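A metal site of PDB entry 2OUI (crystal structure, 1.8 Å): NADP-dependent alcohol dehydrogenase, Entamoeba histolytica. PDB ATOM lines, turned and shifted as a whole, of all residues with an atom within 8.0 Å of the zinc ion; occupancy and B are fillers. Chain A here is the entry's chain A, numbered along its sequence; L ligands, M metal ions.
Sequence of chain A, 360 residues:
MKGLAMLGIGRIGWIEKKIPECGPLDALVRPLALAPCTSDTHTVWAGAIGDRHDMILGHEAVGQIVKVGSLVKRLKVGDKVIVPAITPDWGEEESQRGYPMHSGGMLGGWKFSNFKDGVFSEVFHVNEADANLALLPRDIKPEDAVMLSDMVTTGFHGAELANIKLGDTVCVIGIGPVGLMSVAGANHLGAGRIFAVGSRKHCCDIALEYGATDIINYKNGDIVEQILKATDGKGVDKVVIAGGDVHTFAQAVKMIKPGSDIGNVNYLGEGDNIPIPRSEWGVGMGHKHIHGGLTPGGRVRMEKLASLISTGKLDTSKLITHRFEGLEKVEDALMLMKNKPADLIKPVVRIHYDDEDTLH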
ATOM      1  N   ALA A  35       3.637  22.106 -29.851  1.00  0.00           N
ATOM      2  CA  ALA A  35       4.361  20.870 -30.200  1.00  0.00           C
ATOM      3  C   ALA A  35       5.098  20.333 -28.967  1.00  0.00           C
ATOM      4  O   ALA A  35       5.533  21.121 -28.132  1.00  0.00           O
ATOM      5  CB  ALA A  35       5.351  21.143 -31.333  1.00  0.00           C
ATOM      6  N   PRO A  36       5.221  18.991 -28.853  1.00  0.00           N
ATOM      7  CA  PRO A  36       6.004  18.368 -27.786  1.00  0.00           C
ATOM      8  C   PRO A  36       7.471  18.177 -28.188  1.00  0.00           C
ATOM      9  O   PRO A  36       7.802  18.180 -29.383  1.00  0.00           O
ATOM     10  CB  PRO A  36       5.359  17.006 -27.647  1.00  0.00           C
ATOM     11  CG  PRO A  36       5.027  16.659 -29.090  1.00  0.00           C
ATOM     12  CD  PRO A  36       4.616  17.984 -29.736  1.00  0.00           C
ATOM     13  N   CYS A  37       8.342  18.024 -27.185  1.00  0.00           N
ATOM     14  CA  CYS A  37       9.782  17.963 -27.409  1.00  0.00           C
ATOM     15  C   CYS A  37      10.358  16.764 -26.691  1.00  0.00           C
ATOM     16  O   CYS A  37       9.938  16.450 -25.602  1.00  0.00           O
ATOM     17  CB  CYS A  37      10.463  19.221 -26.864  1.00  0.00           C
ATOM     18  SG  CYS A  37      12.210  19.319 -27.384  1.00  0.00           S
ATOM     19  N   THR A  38      11.330  16.118 -27.314  1.00  0.00           N
ATOM     20  CA  THR A  38      12.138  15.078 -26.688  1.00  0.00           C
ATOM     21  C   THR A  38      12.694  15.538 -25.341  1.00  0.00           C
ATOM     22  O   THR A  38      12.782  14.753 -24.411  1.00  0.00           O
ATOM     23  CB  THR A  38      13.311  14.710 -27.634  1.00  0.00           C
ATOM     24  OG1 THR A  38      12.770  14.356 -28.923  1.00  0.00           O
ATOM     25  CG2 THR A  38      14.072  13.510 -27.107  1.00  0.00           C
ATOM     26  N   SER A  39      13.032  16.817 -25.223  1.00  0.00           N
ATOM     27  CA  SER A  39      13.591  17.314 -23.962  1.00  0.00           C
ATOM     28  C   SER A  39      12.673  17.010 -22.805  1.00  0.00           C
ATOM     29  O   SER A  39      13.121  16.631 -21.716  1.00  0.00           O
ATOM     30  CB  SER A  39      13.862  18.814 -24.018  1.00  0.00           C
ATOM     31  OG  SER A  39      14.804  19.094 -25.032  1.00  0.00           O
ATOM     32  N   ASP A  40      11.370  17.188 -23.004  1.00  0.00           N
ATOM     33  CA  ASP A  40      10.437  16.932 -21.913  1.00  0.00           C
ATOM     34  C   ASP A  40      10.361  15.466 -21.526  1.00  0.00           C
ATOM     35  O   ASP A  40      10.041  15.134 -20.372  1.00  0.00           O
ATOM     36  CB  ASP A  40       9.051  17.474 -22.257  1.00  0.00           C
ATOM     37  CG  ASP A  40       8.927  18.990 -21.983  1.00  0.00           C
ATOM     38  OD1 ASP A  40       9.872  19.611 -21.434  1.00  0.00           O
ATOM     39  OD2 ASP A  40       7.852  19.543 -22.290  1.00  0.00           O
ATOM     40  N   GLY A  58       5.909  21.572 -21.823  1.00  0.00           N
ATOM     41  CA  GLY A  58       5.893  22.229 -23.128  1.00  0.00           C
ATOM     42  C   GLY A  58       6.574  23.584 -23.218  1.00  0.00           C
ATOM     43  O   GLY A  58       6.496  24.421 -22.302  1.00  0.00           O
ATOM     44  N   HIS A  59       7.230  23.818 -24.351  1.00  0.00           N
ATOM     45  CA  HIS A  59       7.935  25.069 -24.577  1.00  0.00           C
ATOM     46  C   HIS A  59       7.973  25.464 -26.061  1.00  0.00           C
ATOM     47  O   HIS A  59       8.872  26.191 -26.495  1.00  0.00           O
ATOM     48  CB  HIS A  59       9.356  25.022 -23.980  1.00  0.00           C
ATOM     49  CG  HIS A  59      10.149  23.790 -24.343  1.00  0.00           C
ATOM     50  ND1 HIS A  59      10.293  22.723 -23.477  1.00  0.00           N
ATOM     51  CD2 HIS A  59      10.839  23.469 -25.464  1.00  0.00           C
ATOM     52  CE1 HIS A  59      11.025  21.792 -24.060  1.00  0.00           C
ATOM     53  NE2 HIS A  59      11.379  22.214 -25.260  1.00  0.00           N
ATOM     54  N   GLU A  60       6.989  24.993 -26.829  1.00  0.00           N
ATOM     55  CA  GLU A  60       6.887  25.316 -28.239  1.00  0.00           C
ATOM     56  C   GLU A  60       5.437  25.705 -28.513  1.00  0.00           C
ATOM     57  O   GLU A  60       4.552  24.867 -28.449  1.00  0.00           O
ATOM     58  CB  GLU A  60       7.247  24.081 -29.057  1.00  0.00           C
ATOM     59  CG  GLU A  60       8.736  23.728 -28.955  1.00  0.00           C
ATOM     60  CD  GLU A  60       9.038  22.332 -29.454  1.00  0.00           C
ATOM     61  OE1 GLU A  60       9.396  22.202 -30.649  1.00  0.00           O
ATOM     62  OE2 GLU A  60       8.862  21.362 -28.665  1.00  0.00           O
ATOM     63  N   ALA A  85      11.087  29.197 -27.207  1.00  0.00           N
ATOM     64  CA  ALA A  85      11.222  28.320 -26.032  1.00  0.00           C
ATOM     65  C   ALA A  85      12.008  29.046 -24.937  1.00  0.00           C
ATOM     66  O   ALA A  85      11.773  28.824 -23.753  1.00  0.00           O
ATOM     67  CB  ALA A  85      11.946  27.006 -26.398  1.00  0.00           C
ATOM     68  N   ILE A  86      12.962  29.896 -25.370  1.00  0.00           N
ATOM     69  CA  ILE A  86      13.858  30.637 -24.459  1.00  0.00           C
ATOM     70  C   ILE A  86      13.375  32.069 -24.409  1.00  0.00           C
ATOM     71  O   ILE A  86      13.231  32.738 -25.447  1.00  0.00           O
ATOM     72  CB  ILE A  86      15.365  30.531 -24.879  1.00  0.00           C
ATOM     73  CG1 ILE A  86      16.006  29.220 -24.353  1.00  0.00           C
ATOM     74  CG2 ILE A  86      16.191  31.690 -24.307  1.00  0.00           C
ATOM     75  CD1 ILE A  86      15.259  27.918 -24.698  1.00  0.00           C
ATOM     76  N   TRP A 110      15.958  29.410 -20.391  1.00  0.00           N
ATOM     77  CA  TRP A 110      14.997  28.360 -20.714  1.00  0.00           C
ATOM     78  C   TRP A 110      14.100  28.156 -19.484  1.00  0.00           C
ATOM     79  O   TRP A 110      14.468  27.444 -18.535  1.00  0.00           O
ATOM     80  CB  TRP A 110      15.707  27.071 -21.131  1.00  0.00           C
ATOM     81  CG  TRP A 110      14.772  25.883 -21.291  1.00  0.00           C
ATOM     82  CD1 TRP A 110      13.440  25.912 -21.653  1.00  0.00           C
ATOM     83  CD2 TRP A 110      15.118  24.505 -21.139  1.00  0.00           C
ATOM     84  NE1 TRP A 110      12.940  24.620 -21.707  1.00  0.00           N
ATOM     85  CE2 TRP A 110      13.933  23.743 -21.370  1.00  0.00           C
ATOM     86  CE3 TRP A 110      16.294  23.831 -20.783  1.00  0.00           C
ATOM     87  CZ2 TRP A 110      13.921  22.353 -21.290  1.00  0.00           C
ATOM     88  CZ3 TRP A 110      16.280  22.454 -20.682  1.00  0.00           C
ATOM     89  CH2 TRP A 110      15.088  21.723 -20.943  1.00  0.00           C
ATOM     90  N   PHE A 112      10.196  27.878 -19.546  1.00  0.00           N
ATOM     91  CA  PHE A 112       9.079  26.974 -19.848  1.00  0.00           C
ATOM     92  C   PHE A 112       9.513  25.496 -19.783  1.00  0.00           C
ATOM     93  O   PHE A 112      10.360  25.076 -20.552  1.00  0.00           O
ATOM     94  CB  PHE A 112       8.568  27.194 -21.270  1.00  0.00           C
ATOM     95  CG  PHE A 112       7.890  28.527 -21.520  1.00  0.00           C
ATOM     96  CD1 PHE A 112       6.889  29.005 -20.670  1.00  0.00           C
ATOM     97  CD2 PHE A 112       8.178  29.233 -22.678  1.00  0.00           C
ATOM     98  CE1 PHE A 112       6.218  30.228 -20.937  1.00  0.00           C
ATOM     99  CE2 PHE A 112       7.514  30.448 -22.958  1.00  0.00           C
ATOM    100  CZ  PHE A 112       6.546  30.941 -22.087  1.00  0.00           C
ATOM    101  N   SER A 113       8.878  24.723 -18.900  1.00  0.00           N
ATOM    102  CA  SER A 113       9.136  23.275 -18.717  1.00  0.00           C
ATOM    103  C   SER A 113      10.575  22.962 -18.284  1.00  0.00           C
ATOM    104  O   SER A 113      10.975  21.802 -18.298  1.00  0.00           O
ATOM    105  CB  SER A 113       8.679  22.387 -19.901  1.00  0.00           C
ATOM    106  OG  SER A 113       9.680  22.249 -20.916  1.00  0.00           O
ATOM    107  N   SER A 149      10.107  27.935 -32.617  1.00  0.00           N
ATOM    108  CA  SER A 149      10.255  28.182 -31.177  1.00  0.00           C
ATOM    109  C   SER A 149      11.478  27.493 -30.600  1.00  0.00           C
ATOM    110  O   SER A 149      12.137  28.052 -29.725  1.00  0.00           O
ATOM    111  CB  SER A 149       9.020  27.622 -30.448  1.00  0.00           C
ATOM    112  OG  SER A 149       7.841  28.263 -30.909  1.00  0.00           O
ATOM    113  N   ASP A 150      11.747  26.303 -31.116  1.00  0.00           N
ATOM    114  CA  ASP A 150      12.754  25.397 -30.551  1.00  0.00           C
ATOM    115  C   ASP A 150      13.461  24.663 -31.688  1.00  0.00           C
ATOM    116  O   ASP A 150      14.681  24.676 -31.747  1.00  0.00           O
ATOM    117  CB  ASP A 150      12.067  24.445 -29.575  1.00  0.00           C
ATOM    118  CG  ASP A 150      13.040  23.590 -28.744  1.00  0.00           C
ATOM    119  OD1 ASP A 150      14.274  23.822 -28.791  1.00  0.00           O
ATOM    120  OD2 ASP A 150      12.521  22.656 -28.058  1.00  0.00           O
ATOM    121  N   MET A 151      12.730  24.054 -32.633  1.00  0.00           N
ATOM    122  CA  MET A 151      13.413  23.167 -33.600  1.00  0.00           C
ATOM    123  C   MET A 151      14.358  23.905 -34.543  1.00  0.00           C
ATOM    124  O   MET A 151      15.528  23.565 -34.649  1.00  0.00           O
ATOM    125  CB  MET A 151      12.439  22.303 -34.391  1.00  0.00           C
ATOM    126  CG  MET A 151      11.541  21.393 -33.510  1.00  0.00           C
ATOM    127  SD  MET A 151      12.489  20.159 -32.598  1.00  0.00           S
ATOM    128  CE  MET A 151      12.785  20.936 -31.005  1.00  0.00           C
ATOM    129  N   THR A 154      17.185  25.881 -32.344  1.00  0.00           N
ATOM    130  CA  THR A 154      18.190  24.989 -31.745  1.00  0.00           C
ATOM    131  C   THR A 154      19.032  24.316 -32.827  1.00  0.00           C
ATOM    132  O   THR A 154      20.257  24.264 -32.713  1.00  0.00           O
ATOM    133  CB  THR A 154      17.521  23.944 -30.849  1.00  0.00           C
ATOM    134  OG1 THR A 154      16.754  24.634 -29.852  1.00  0.00           O
ATOM    135  CG2 THR A 154      18.577  23.071 -30.172  1.00  0.00           C
ATOM    136  N   VAL A 178      15.513  18.344 -34.564  1.00  0.00           N
ATOM    137  CA  VAL A 178      16.591  19.316 -34.322  1.00  0.00           C
ATOM    138  C   VAL A 178      17.730  19.100 -35.290  1.00  0.00           C
ATOM    139  O   VAL A 178      18.201  20.063 -35.900  1.00  0.00           O
ATOM    140  CB  VAL A 178      17.129  19.288 -32.867  1.00  0.00           C
ATOM    141  CG1 VAL A 178      18.387  20.239 -32.665  1.00  0.00           C
ATOM    142  CG2 VAL A 178      16.032  19.720 -31.908  1.00  0.00           C
ATOM    143  N   TYR A 267      20.493  17.798 -25.630  1.00  0.00           N
ATOM    144  CA  TYR A 267      20.280  17.749 -24.192  1.00  0.00           C
ATOM    145  C   TYR A 267      20.583  16.313 -23.733  1.00  0.00           C
ATOM    146  O   TYR A 267      19.870  15.360 -24.101  1.00  0.00           O
ATOM    147  CB  TYR A 267      18.843  18.189 -23.929  1.00  0.00           C
ATOM    148  CG  TYR A 267      18.214  17.965 -22.548  1.00  0.00           C
ATOM    149  CD1 TYR A 267      16.847  18.146 -22.407  1.00  0.00           C
ATOM    150  CD2 TYR A 267      18.959  17.559 -21.428  1.00  0.00           C
ATOM    151  CE1 TYR A 267      16.227  17.960 -21.191  1.00  0.00           C
ATOM    152  CE2 TYR A 267      18.311  17.352 -20.175  1.00  0.00           C
ATOM    153  CZ  TYR A 267      16.941  17.579 -20.094  1.00  0.00           C
ATOM    154  OH  TYR A 267      16.234  17.397 -18.913  1.00  0.00           O
ATOM    155  N   LEU A 294      22.704  25.854 -25.174  1.00  0.00           N
ATOM    156  CA  LEU A 294      21.265  26.148 -25.230  1.00  0.00           C
ATOM    157  C   LEU A 294      20.881  27.188 -26.293  1.00  0.00           C
ATOM    158  O   LEU A 294      21.575  28.187 -26.479  1.00  0.00           O
ATOM    159  CB  LEU A 294      20.868  26.658 -23.833  1.00  0.00           C
ATOM    160  CG  LEU A 294      19.394  26.963 -23.578  1.00  0.00           C
ATOM    161  CD1 LEU A 294      18.514  25.730 -23.737  1.00  0.00           C
ATOM    162  CD2 LEU A 294      19.267  27.578 -22.192  1.00  0.00           C
ATOM    163  N   THR A 295      19.767  26.990 -27.004  1.00  0.00           N
ATOM    164  CA  THR A 295      19.384  27.928 -28.070  1.00  0.00           C
ATOM    165  C   THR A 295      19.207  29.373 -27.587  1.00  0.00           C
ATOM    166  O   THR A 295      18.737  29.603 -26.461  1.00  0.00           O
ATOM    167  CB  THR A 295      18.081  27.459 -28.762  1.00  0.00           C
ATOM    168  OG1 THR A 295      17.704  28.404 -29.778  1.00  0.00           O
ATOM    169  CG2 THR A 295      16.953  27.274 -27.725  1.00  0.00           C
ATOM    170  N   MET A 337       6.531  11.310 -28.532  1.00  0.00           N
ATOM    171  CA  MET A 337       7.940  11.680 -28.422  1.00  0.00           C
ATOM    172  C   MET A 337       8.691  10.698 -27.544  1.00  0.00           C
ATOM    173  O   MET A 337       9.925  10.511 -27.692  1.00  0.00           O
ATOM    174  CB  MET A 337       8.117  13.096 -27.866  1.00  0.00           C
ATOM    175  CG  MET A 337       7.463  14.187 -28.692  1.00  0.00           C
ATOM    176  SD  MET A 337       7.969  14.188 -30.431  1.00  0.00           S
ATOM    177  CE  MET A 337       9.464  15.155 -30.399  1.00  0.00           C
ATOM    178  N   LYS A 346       7.897  15.242 -35.968  1.00  0.00           N
ATOM    179  CA  LYS A 346       7.365  16.201 -34.997  1.00  0.00           C
ATOM    180  C   LYS A 346       5.839  16.265 -35.099  1.00  0.00           C
ATOM    181  O   LYS A 346       5.302  16.430 -36.186  1.00  0.00           O
ATOM    182  CB  LYS A 346       8.005  17.563 -35.306  1.00  0.00           C
ATOM    183  CG  LYS A 346       7.902  18.583 -34.222  1.00  0.00           C
ATOM    184  CD  LYS A 346       8.862  18.328 -33.087  1.00  0.00           C
ATOM    185  CE  LYS A 346       8.716  19.486 -32.124  1.00  0.00           C
ATOM    186  NZ  LYS A 346       9.608  19.360 -30.938  1.00  0.00           N
HETATM  187 AS1  LIG L   1      15.455  22.604 -25.748  1.00  0.00          AS
HETATM  188  O1  LIG L   1      16.137  22.654 -27.340  1.00  0.00           O
HETATM  189  O2  LIG L   1      14.242  21.332 -25.629  1.00  0.00           O
HETATM  190  C1  LIG L   1      16.776  22.073 -24.399  1.00  0.00           C
HETATM  191  C2  LIG L   1      14.600  24.308 -25.288  1.00  0.00           C
HETATM  192 ZN    ZN M   1      12.630  21.406 -26.688  1.00  0.00          ZN
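Ser 39 touches the zinc ion (OG to ZN, 3.6 Å). The nearest printed residue that does not touch the zinc ion is Glu 60 (4.3 Å).
OG1 of Thr 154 is in hydrogen-bond range of O of Asp 150. The side-chain hydroxyl (OG) of Ser 113 is in hydrogen-bond range of a ring nitrogen (ND1) of His 59 (2.7 Å). N of Ser 39 lies close to SG of Cys 37, 3.4 Å away.
The zinc ion is bound by OD2 of Asp 150 (1.9 Å), O2 of the ligand (1.9 Å), NE2 of His 59 (2.1 Å) and SG of Cys 37 (2.2 Å).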
